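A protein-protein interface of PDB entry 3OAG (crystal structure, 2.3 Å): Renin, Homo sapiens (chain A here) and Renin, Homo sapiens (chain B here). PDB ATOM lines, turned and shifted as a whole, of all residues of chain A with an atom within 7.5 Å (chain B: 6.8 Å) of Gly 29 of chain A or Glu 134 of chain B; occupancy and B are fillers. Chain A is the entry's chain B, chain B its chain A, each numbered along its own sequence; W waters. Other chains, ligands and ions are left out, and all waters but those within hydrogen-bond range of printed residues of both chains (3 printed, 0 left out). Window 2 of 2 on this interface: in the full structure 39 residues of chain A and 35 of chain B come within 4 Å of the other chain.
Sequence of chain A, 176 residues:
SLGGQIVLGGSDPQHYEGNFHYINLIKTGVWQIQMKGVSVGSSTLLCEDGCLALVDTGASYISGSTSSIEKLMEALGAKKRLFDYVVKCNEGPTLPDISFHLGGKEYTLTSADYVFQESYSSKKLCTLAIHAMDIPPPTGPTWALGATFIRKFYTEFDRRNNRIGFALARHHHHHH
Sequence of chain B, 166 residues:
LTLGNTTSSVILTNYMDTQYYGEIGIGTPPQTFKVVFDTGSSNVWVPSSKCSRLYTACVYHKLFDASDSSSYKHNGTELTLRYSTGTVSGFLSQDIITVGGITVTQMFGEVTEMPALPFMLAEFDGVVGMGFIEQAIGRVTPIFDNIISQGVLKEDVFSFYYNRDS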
ATOM      1  N   LEU A  25     -17.785 -12.152  -7.728  1.00  0.00           N
ATOM      2  CA  LEU A  25     -16.963 -12.720  -8.784  1.00  0.00           C
ATOM      3  C   LEU A  25     -17.840 -13.612  -9.663  1.00  0.00           C
ATOM      4  O   LEU A  25     -18.851 -14.151  -9.198  1.00  0.00           O
ATOM      5  CB  LEU A  25     -15.787 -13.508  -8.201  1.00  0.00           C
ATOM      6  CG  LEU A  25     -14.841 -12.842  -7.187  1.00  0.00           C
ATOM      7  CD1 LEU A  25     -13.702 -13.796  -6.853  1.00  0.00           C
ATOM      8  CD2 LEU A  25     -14.297 -11.502  -7.682  1.00  0.00           C
ATOM      9  N   LYS A  27     -16.790 -16.472 -11.336  1.00  0.00           N
ATOM     10  CA  LYS A  27     -16.442 -17.757 -10.751  1.00  0.00           C
ATOM     11  C   LYS A  27     -15.251 -17.532  -9.834  1.00  0.00           C
ATOM     12  O   LYS A  27     -14.360 -16.729 -10.151  1.00  0.00           O
ATOM     13  CB  LYS A  27     -16.081 -18.778 -11.836  1.00  0.00           C
ATOM     14  CG  LYS A  27     -15.155 -18.249 -12.939  1.00  0.00           C
ATOM     15  CD  LYS A  27     -14.198 -19.326 -13.438  1.00  0.00           C
ATOM     16  CE  LYS A  27     -13.868 -19.139 -14.917  1.00  0.00           C
ATOM     17  NZ  LYS A  27     -13.128 -17.871 -15.209  1.00  0.00           N
ATOM     18  N   THR A  28     -15.241 -18.215  -8.689  1.00  0.00           N
ATOM     19  CA  THR A  28     -14.072 -18.205  -7.818  1.00  0.00           C
ATOM     20  C   THR A  28     -12.894 -18.747  -8.628  1.00  0.00           C
ATOM     21  O   THR A  28     -13.088 -19.430  -9.636  1.00  0.00           O
ATOM     22  CB  THR A  28     -14.299 -18.998  -6.490  1.00  0.00           C
ATOM     23  OG1 THR A  28     -13.238 -18.712  -5.563  1.00  0.00           O
ATOM     24  CG2 THR A  28     -14.391 -20.514  -6.730  1.00  0.00           C
ATOM     25  N   GLY A  29     -11.679 -18.407  -8.225  1.00  0.00           N
ATOM     26  CA  GLY A  29     -10.516 -18.814  -8.993  1.00  0.00           C
ATOM     27  C   GLY A  29      -9.843 -17.680  -9.740  1.00  0.00           C
ATOM     28  O   GLY A  29      -8.702 -17.817 -10.163  1.00  0.00           O
ATOM     29  N   VAL A  30     -10.548 -16.564  -9.894  1.00  0.00           N
ATOM     30  CA  VAL A  30     -10.006 -15.374 -10.547  1.00  0.00           C
ATOM     31  C   VAL A  30     -10.679 -14.091 -10.039  1.00  0.00           C
ATOM     32  O   VAL A  30     -11.873 -14.094  -9.712  1.00  0.00           O
ATOM     33  CB  VAL A  30     -10.100 -15.482 -12.084  1.00  0.00           C
ATOM     34  CG1 VAL A  30     -11.539 -15.661 -12.536  1.00  0.00           C
ATOM     35  CG2 VAL A  30      -9.448 -14.274 -12.759  1.00  0.00           C
ATOM     36  N   TRP A  31      -9.910 -13.005  -9.961  1.00  0.00           N
ATOM     37  CA  TRP A  31     -10.447 -11.733  -9.502  1.00  0.00           C
ATOM     38  C   TRP A  31     -11.096 -10.978 -10.664  1.00  0.00           C
ATOM     39  O   TRP A  31     -10.675  -9.875 -11.017  1.00  0.00           O
ATOM     40  CB  TRP A  31      -9.372 -10.887  -8.830  1.00  0.00           C
ATOM     41  CG  TRP A  31      -8.908 -11.407  -7.522  1.00  0.00           C
ATOM     42  CD1 TRP A  31      -7.672 -11.903  -7.234  1.00  0.00           C
ATOM     43  CD2 TRP A  31      -9.663 -11.468  -6.298  1.00  0.00           C
ATOM     44  NE1 TRP A  31      -7.608 -12.273  -5.916  1.00  0.00           N
ATOM     45  CE2 TRP A  31      -8.814 -12.023  -5.317  1.00  0.00           C
ATOM     46  CE3 TRP A  31     -10.976 -11.120  -5.940  1.00  0.00           C
ATOM     47  CZ2 TRP A  31      -9.228 -12.227  -3.998  1.00  0.00           C
ATOM     48  CZ3 TRP A  31     -11.392 -11.330  -4.630  1.00  0.00           C
ATOM     49  CH2 TRP A  31     -10.520 -11.882  -3.676  1.00  0.00           C
ATOM     50  N   GLN A  32     -12.144 -11.582 -11.222  1.00  0.00           N
ATOM     51  CA  GLN A  32     -12.849 -11.067 -12.383  1.00  0.00           C
ATOM     52  C   GLN A  32     -14.341 -10.930 -12.073  1.00  0.00           C
ATOM     53  O   GLN A  32     -14.930 -11.805 -11.433  1.00  0.00           O
ATOM     54  CB  GLN A  32     -12.626 -12.012 -13.560  1.00  0.00           C
ATOM     55  CG  GLN A  32     -13.066 -11.522 -14.921  1.00  0.00           C
ATOM     56  CD  GLN A  32     -12.615 -12.477 -16.017  1.00  0.00           C
ATOM     57  OE1 GLN A  32     -12.039 -12.067 -17.030  1.00  0.00           O
ATOM     58  NE2 GLN A  32     -12.843 -13.762 -15.800  1.00  0.00           N
ATOM     59  N   PRO A 138      -8.020 -19.106 -20.377  1.00  0.00           N
ATOM     60  CA  PRO A 138      -9.394 -19.001 -19.864  1.00  0.00           C
ATOM     61  C   PRO A 138      -9.796 -17.613 -19.350  1.00  0.00           C
ATOM     62  O   PRO A 138     -10.966 -17.239 -19.474  1.00  0.00           O
ATOM     63  CB  PRO A 138      -9.412 -20.011 -18.714  1.00  0.00           C
ATOM     64  CG  PRO A 138      -8.006 -20.032 -18.209  1.00  0.00           C
ATOM     65  CD  PRO A 138      -7.104 -19.685 -19.372  1.00  0.00           C
ATOM     66  N   THR A 139      -8.845 -16.865 -18.789  1.00  0.00           N
ATOM     67  CA  THR A 139      -9.143 -15.563 -18.188  1.00  0.00           C
ATOM     68  C   THR A 139      -9.904 -14.647 -19.152  1.00  0.00           C
ATOM     69  O   THR A 139     -10.981 -14.149 -18.816  1.00  0.00           O
ATOM     70  CB  THR A 139      -7.876 -14.842 -17.692  1.00  0.00           C
ATOM     71  OG1 THR A 139      -7.094 -15.736 -16.892  1.00  0.00           O
ATOM     72  CG2 THR A 139      -8.249 -13.631 -16.865  1.00  0.00           C
ATOM     73  N   ARG A 159     -12.061 -12.497   0.188  1.00  0.00           N
ATOM     74  CA  ARG A 159     -11.969 -13.944  -0.067  1.00  0.00           C
ATOM     75  C   ARG A 159     -13.037 -14.736   0.685  1.00  0.00           C
ATOM     76  O   ARG A 159     -13.471 -15.803   0.240  1.00  0.00           O
ATOM     77  CB  ARG A 159     -10.572 -14.465   0.296  1.00  0.00           C
ATOM     78  CG  ARG A 159      -9.508 -14.187  -0.744  1.00  0.00           C
ATOM     79  CD  ARG A 159      -9.661 -15.050  -1.981  1.00  0.00           C
ATOM     80  NE  ARG A 159      -9.581 -16.485  -1.692  1.00  0.00           N
ATOM     81  CZ  ARG A 159      -8.454 -17.191  -1.639  1.00  0.00           C
ATOM     82  NH1 ARG A 159      -7.272 -16.618  -1.859  1.00  0.00           N
ATOM     83  NH2 ARG A 159      -8.508 -18.481  -1.360  1.00  0.00           N
ATOM     84  N   ASN A 162     -16.114 -13.944  -1.585  1.00  0.00           N
ATOM     85  CA  ASN A 162     -15.815 -13.900  -3.022  1.00  0.00           C
ATOM     86  C   ASN A 162     -16.400 -12.668  -3.711  1.00  0.00           C
ATOM     87  O   ASN A 162     -17.179 -12.769  -4.664  1.00  0.00           O
ATOM     88  CB  ASN A 162     -16.252 -15.177  -3.739  1.00  0.00           C
ATOM     89  CG  ASN A 162     -15.363 -16.357  -3.426  1.00  0.00           C
ATOM     90  OD1 ASN A 162     -14.206 -16.417  -3.862  1.00  0.00           O
ATOM     91  ND2 ASN A 162     -15.903 -17.322  -2.683  1.00  0.00           N
ATOM     92  N   SER B  42      -0.875 -15.425  -9.275  1.00  0.00           N
ATOM     93  CA  SER B  42      -1.030 -16.171  -8.014  1.00  0.00           C
ATOM     94  C   SER B  42       0.283 -16.680  -7.421  1.00  0.00           C
ATOM     95  O   SER B  42       0.277 -17.298  -6.369  1.00  0.00           O
ATOM     96  CB  SER B  42      -1.973 -17.366  -8.204  1.00  0.00           C
ATOM     97  OG  SER B  42      -3.171 -16.993  -8.849  1.00  0.00           O
ATOM     98  N   GLY B 131      -3.746 -13.637  -6.407  1.00  0.00           N
ATOM     99  CA  GLY B 131      -4.836 -14.388  -7.004  1.00  0.00           C
ATOM    100  C   GLY B 131      -4.934 -15.785  -6.406  1.00  0.00           C
ATOM    101  O   GLY B 131      -4.262 -16.090  -5.424  1.00  0.00           O
ATOM    102  N   PHE B 132      -5.752 -16.629  -7.033  1.00  0.00           N
ATOM    103  CA  PHE B 132      -6.208 -17.893  -6.454  1.00  0.00           C
ATOM    104  C   PHE B 132      -5.328 -19.058  -6.883  1.00  0.00           C
ATOM    105  O   PHE B 132      -4.709 -19.024  -7.949  1.00  0.00           O
ATOM    106  CB  PHE B 132      -7.659 -18.190  -6.890  1.00  0.00           C
ATOM    107  CG  PHE B 132      -8.677 -17.163  -6.431  1.00  0.00           C
ATOM    108  CD1 PHE B 132      -8.860 -15.966  -7.132  1.00  0.00           C
ATOM    109  CD2 PHE B 132      -9.477 -17.411  -5.325  1.00  0.00           C
ATOM    110  CE1 PHE B 132      -9.804 -15.034  -6.718  1.00  0.00           C
ATOM    111  CE2 PHE B 132     -10.428 -16.483  -4.905  1.00  0.00           C
ATOM    112  CZ  PHE B 132     -10.588 -15.292  -5.594  1.00  0.00           C
ATOM    113  N   ILE B 133      -5.312 -20.102  -6.062  1.00  0.00           N
ATOM    114  CA  ILE B 133      -4.575 -21.330  -6.359  1.00  0.00           C
ATOM    115  C   ILE B 133      -4.879 -21.907  -7.750  1.00  0.00           C
ATOM    116  O   ILE B 133      -4.002 -22.500  -8.383  1.00  0.00           O
ATOM    117  CB  ILE B 133      -4.767 -22.394  -5.240  1.00  0.00           C
ATOM    118  CG1 ILE B 133      -3.676 -23.471  -5.326  1.00  0.00           C
ATOM    119  CG2 ILE B 133      -6.186 -22.964  -5.241  1.00  0.00           C
ATOM    120  CD1 ILE B 133      -3.532 -24.309  -4.059  1.00  0.00           C
ATOM    121  N   GLU B 134      -6.104 -21.688  -8.228  1.00  0.00           N
ATOM    122  CA  GLU B 134      -6.534 -22.143  -9.554  1.00  0.00           C
ATOM    123  C   GLU B 134      -5.628 -21.657 -10.686  1.00  0.00           C
ATOM    124  O   GLU B 134      -5.444 -22.357 -11.679  1.00  0.00           O
ATOM    125  CB  GLU B 134      -7.980 -21.726  -9.825  1.00  0.00           C
ATOM    126  CG  GLU B 134      -9.032 -22.588  -9.131  1.00  0.00           C
ATOM    127  CD  GLU B 134      -9.415 -22.090  -7.750  1.00  0.00           C
ATOM    128  OE1 GLU B 134      -8.593 -21.434  -7.082  1.00  0.00           O
ATOM    129  OE2 GLU B 134     -10.552 -22.362  -7.316  1.00  0.00           O
ATOM    130  N   GLN B 135      -5.061 -20.462 -10.525  1.00  0.00           N
ATOM    131  CA  GLN B 135      -4.221 -19.851 -11.560  1.00  0.00           C
ATOM    132  C   GLN B 135      -2.737 -19.887 -11.203  1.00  0.00           C
ATOM    133  O   GLN B 135      -1.909 -19.311 -11.915  1.00  0.00           O
ATOM    134  CB  GLN B 135      -4.652 -18.408 -11.801  1.00  0.00           C
ATOM    135  CG  GLN B 135      -6.150 -18.221 -11.920  1.00  0.00           C
ATOM    136  CD  GLN B 135      -6.633 -18.292 -13.347  1.00  0.00           C
ATOM    137  OE1 GLN B 135      -6.281 -17.444 -14.173  1.00  0.00           O
ATOM    138  NE2 GLN B 135      -7.461 -19.295 -13.649  1.00  0.00           N
ATOM    139  N   ALA B 136      -2.417 -20.564 -10.100  1.00  0.00           N
ATOM    140  CA  ALA B 136      -1.046 -20.719  -9.636  1.00  0.00           C
ATOM    141  C   ALA B 136      -0.310 -21.745 -10.480  1.00  0.00           C
ATOM    142  O   ALA B 136      -0.787 -22.867 -10.675  1.00  0.00           O
ATOM    143  CB  ALA B 136      -1.033 -21.124  -8.163  1.00  0.00           C
ATOM    144  N   ILE B 137       0.849 -21.354 -10.993  1.00  0.00           N
ATOM    145  CA  ILE B 137       1.708 -22.272 -11.728  1.00  0.00           C
ATOM    146  C   ILE B 137       2.271 -23.306 -10.748  1.00  0.00           C
ATOM    147  O   ILE B 137       2.865 -22.940  -9.734  1.00  0.00           O
ATOM    148  CB  ILE B 137       2.844 -21.510 -12.452  1.00  0.00           C
ATOM    149  CG1 ILE B 137       2.246 -20.420 -13.359  1.00  0.00           C
ATOM    150  CG2 ILE B 137       3.729 -22.466 -13.255  1.00  0.00           C
ATOM    151  CD1 ILE B 137       3.268 -19.631 -14.144  1.00  0.00           C
ATOM    152  N   ARG B 139       0.305 -25.397  -9.135  1.00  0.00           N
ATOM    153  CA  ARG B 139      -0.643 -25.316  -8.019  1.00  0.00           C
ATOM    154  C   ARG B 139       0.046 -25.085  -6.654  1.00  0.00           C
ATOM    155  O   ARG B 139      -0.299 -25.702  -5.642  1.00  0.00           O
ATOM    156  CB  ARG B 139      -1.606 -26.514  -8.005  1.00  0.00           C
ATOM    157  CG  ARG B 139      -2.988 -26.185  -7.407  1.00  0.00           C
ATOM    158  CD  ARG B 139      -3.927 -27.404  -7.341  1.00  0.00           C
ATOM    159  NE  ARG B 139      -5.353 -27.039  -7.293  1.00  0.00           N
ATOM    160  CZ  ARG B 139      -6.032 -26.490  -8.309  1.00  0.00           C
ATOM    161  NH1 ARG B 139      -5.423 -26.202  -9.461  1.00  0.00           N
ATOM    162  NH2 ARG B 139      -7.323 -26.210  -8.171  1.00  0.00           N
ATOM    163  N   PRO B 142      -0.867 -20.079  -2.867  1.00  0.00           N
ATOM    164  CA  PRO B 142      -0.615 -18.642  -2.882  1.00  0.00           C
ATOM    165  C   PRO B 142      -0.417 -18.115  -1.484  1.00  0.00           C
ATOM    166  O   PRO B 142      -0.974 -18.666  -0.530  1.00  0.00           O
ATOM    167  CB  PRO B 142      -1.893 -18.067  -3.498  1.00  0.00           C
ATOM    168  CG  PRO B 142      -2.452 -19.195  -4.283  1.00  0.00           C
ATOM    169  CD  PRO B 142      -2.200 -20.386  -3.415  1.00  0.00           C
ATOM    170  N   ASP B 145      -3.410 -17.382   0.819  1.00  0.00           N
ATOM    171  CA  ASP B 145      -4.005 -18.615   1.334  1.00  0.00           C
ATOM    172  C   ASP B 145      -3.257 -19.153   2.551  1.00  0.00           C
ATOM    173  O   ASP B 145      -3.863 -19.722   3.450  1.00  0.00           O
ATOM    174  CB  ASP B 145      -4.067 -19.674   0.239  1.00  0.00           C
ATOM    175  CG  ASP B 145      -4.991 -19.280  -0.890  1.00  0.00           C
ATOM    176  OD1 ASP B 145      -4.825 -18.173  -1.454  1.00  0.00           O
ATOM    177  OD2 ASP B 145      -5.892 -20.079  -1.209  1.00  0.00           O
HETATM  178  O   HOH W   1      -6.539 -19.829  -3.630  1.00  0.00           O
HETATM  179  O   HOH W   2      -6.621 -15.568  -9.442  1.00  0.00           O
HETATM  180  O   HOH W   3      -4.377 -15.706  -2.891  1.00  0.00           O
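The side-chain hydroxyl (OG1) of Thr 139 of chain A sits at hydrogen-bond distance from the side-chain amide oxygen (OE1) of Gln 135 of chain B, at 3.3 Å. The side-chain carboxylate of Asp 145 of chain B lies within salt-bridge range of the guanidinium group of Arg 159 of chain A, 2.9 Å away.
N of Leu 25 of chain A sits at hydrogen-bond distance from O of Asn 162 of chain A (3.2 Å). The side-chain amide oxygen of Gln 32 of chain A sits close to the backbone carbonyl oxygen of Thr 139 of chain A. The side-chain hydroxyl of Thr 28 of chain A lies within hydrogen-bond range of the side-chain amide oxygen of Asn 162 of chain A (3.0 Å). The side-chain hydroxyl (OG) of Ser 42 of chain B sits at hydrogen-bond distance from the backbone carbonyl oxygen (O) of Phe 132 of chain B (2.7 Å).
Among the printed residues, pairs that only touch across the chains: Leu 25 of chain A with Phe 132 of chain B (3.7 Å), Thr 28 of chain A with Phe 132 of chain B (3.6 Å), Gly 29 of chain A with Phe 132 of chain B (3.3 Å), Gly 29 of chain A with Glu 134 of chain B (3.7 Å), Gly 29 of chain A with Gln 135 of chain B (3.1 Å), Val 30 of chain A with Phe 132 of chain B (3.3 Å), Trp 31 of chain A with Gly 131 of chain B (3.7 Å), Trp 31 of chain A with Phe 132 of chain B (3.5 Å), Arg 159 of chain A with Phe 132 of chain B (3.3 Å) and Asn 162 of chain A with Phe 132 of chain B (3.9 Å).
Gly 29 of chain A touches just these residues of chain B: Phe 132, Glu 134 and Gln 135. Of chain A, only Gly 29 comes within 4 Å of Glu 134 of chain B. Of the printed residues of chain B, Val 30 of chain A touches Phe 132 (3.3 Å). Printed residues of chain A within 4 Å of Phe 132 of chain B: Leu 25 (3.7 Å), Thr 28 (3.6 Å), Gly 29 (3.3 Å), Val 30 (3.3 Å), Trp 31 (3.5 Å), Arg 159 (3.3 Å) and Asn 162 (3.9 Å). The nearest printed residue of chain B that does not touch Thr 139 of chain A is Glu 134 of chain B (8.6 Å).
Of the 11 printed residues of chain A, 8 touch a printed residue of chain B. Hydrophobic or aromatic side chains of chain A that line the printed part of chain B: Leu 25 and Trp 31. Printed residues of chain B that touch a printed residue of chain A: Gly 131, Phe 132, Glu 134, Gln 135 and Asp 145. Among the printed residues, Asp or Glu carboxylates within 4 Å of a Lys or Arg side-chain nitrogen of the other chain: Arg 159 of chain A with Asp 145 of chain B.
Water W1 lies within hydrogen-bond range of OD2 of Asp 145 of chain B, N of Ile 133 of chain B and NH2 of Arg 159 of chain A. Water W3 lies within hydrogen-bond range of O of Gly 131 of chain B (2.6 Å), OD1 of Asp 145 of chain B (2.9 Å) and NH1 of Arg 159 of chain A (3.2 Å). Water W2 bridges N of Phe 132 of chain B (2.8 Å) and O of Gly 29 of chain A (3.1 Å).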
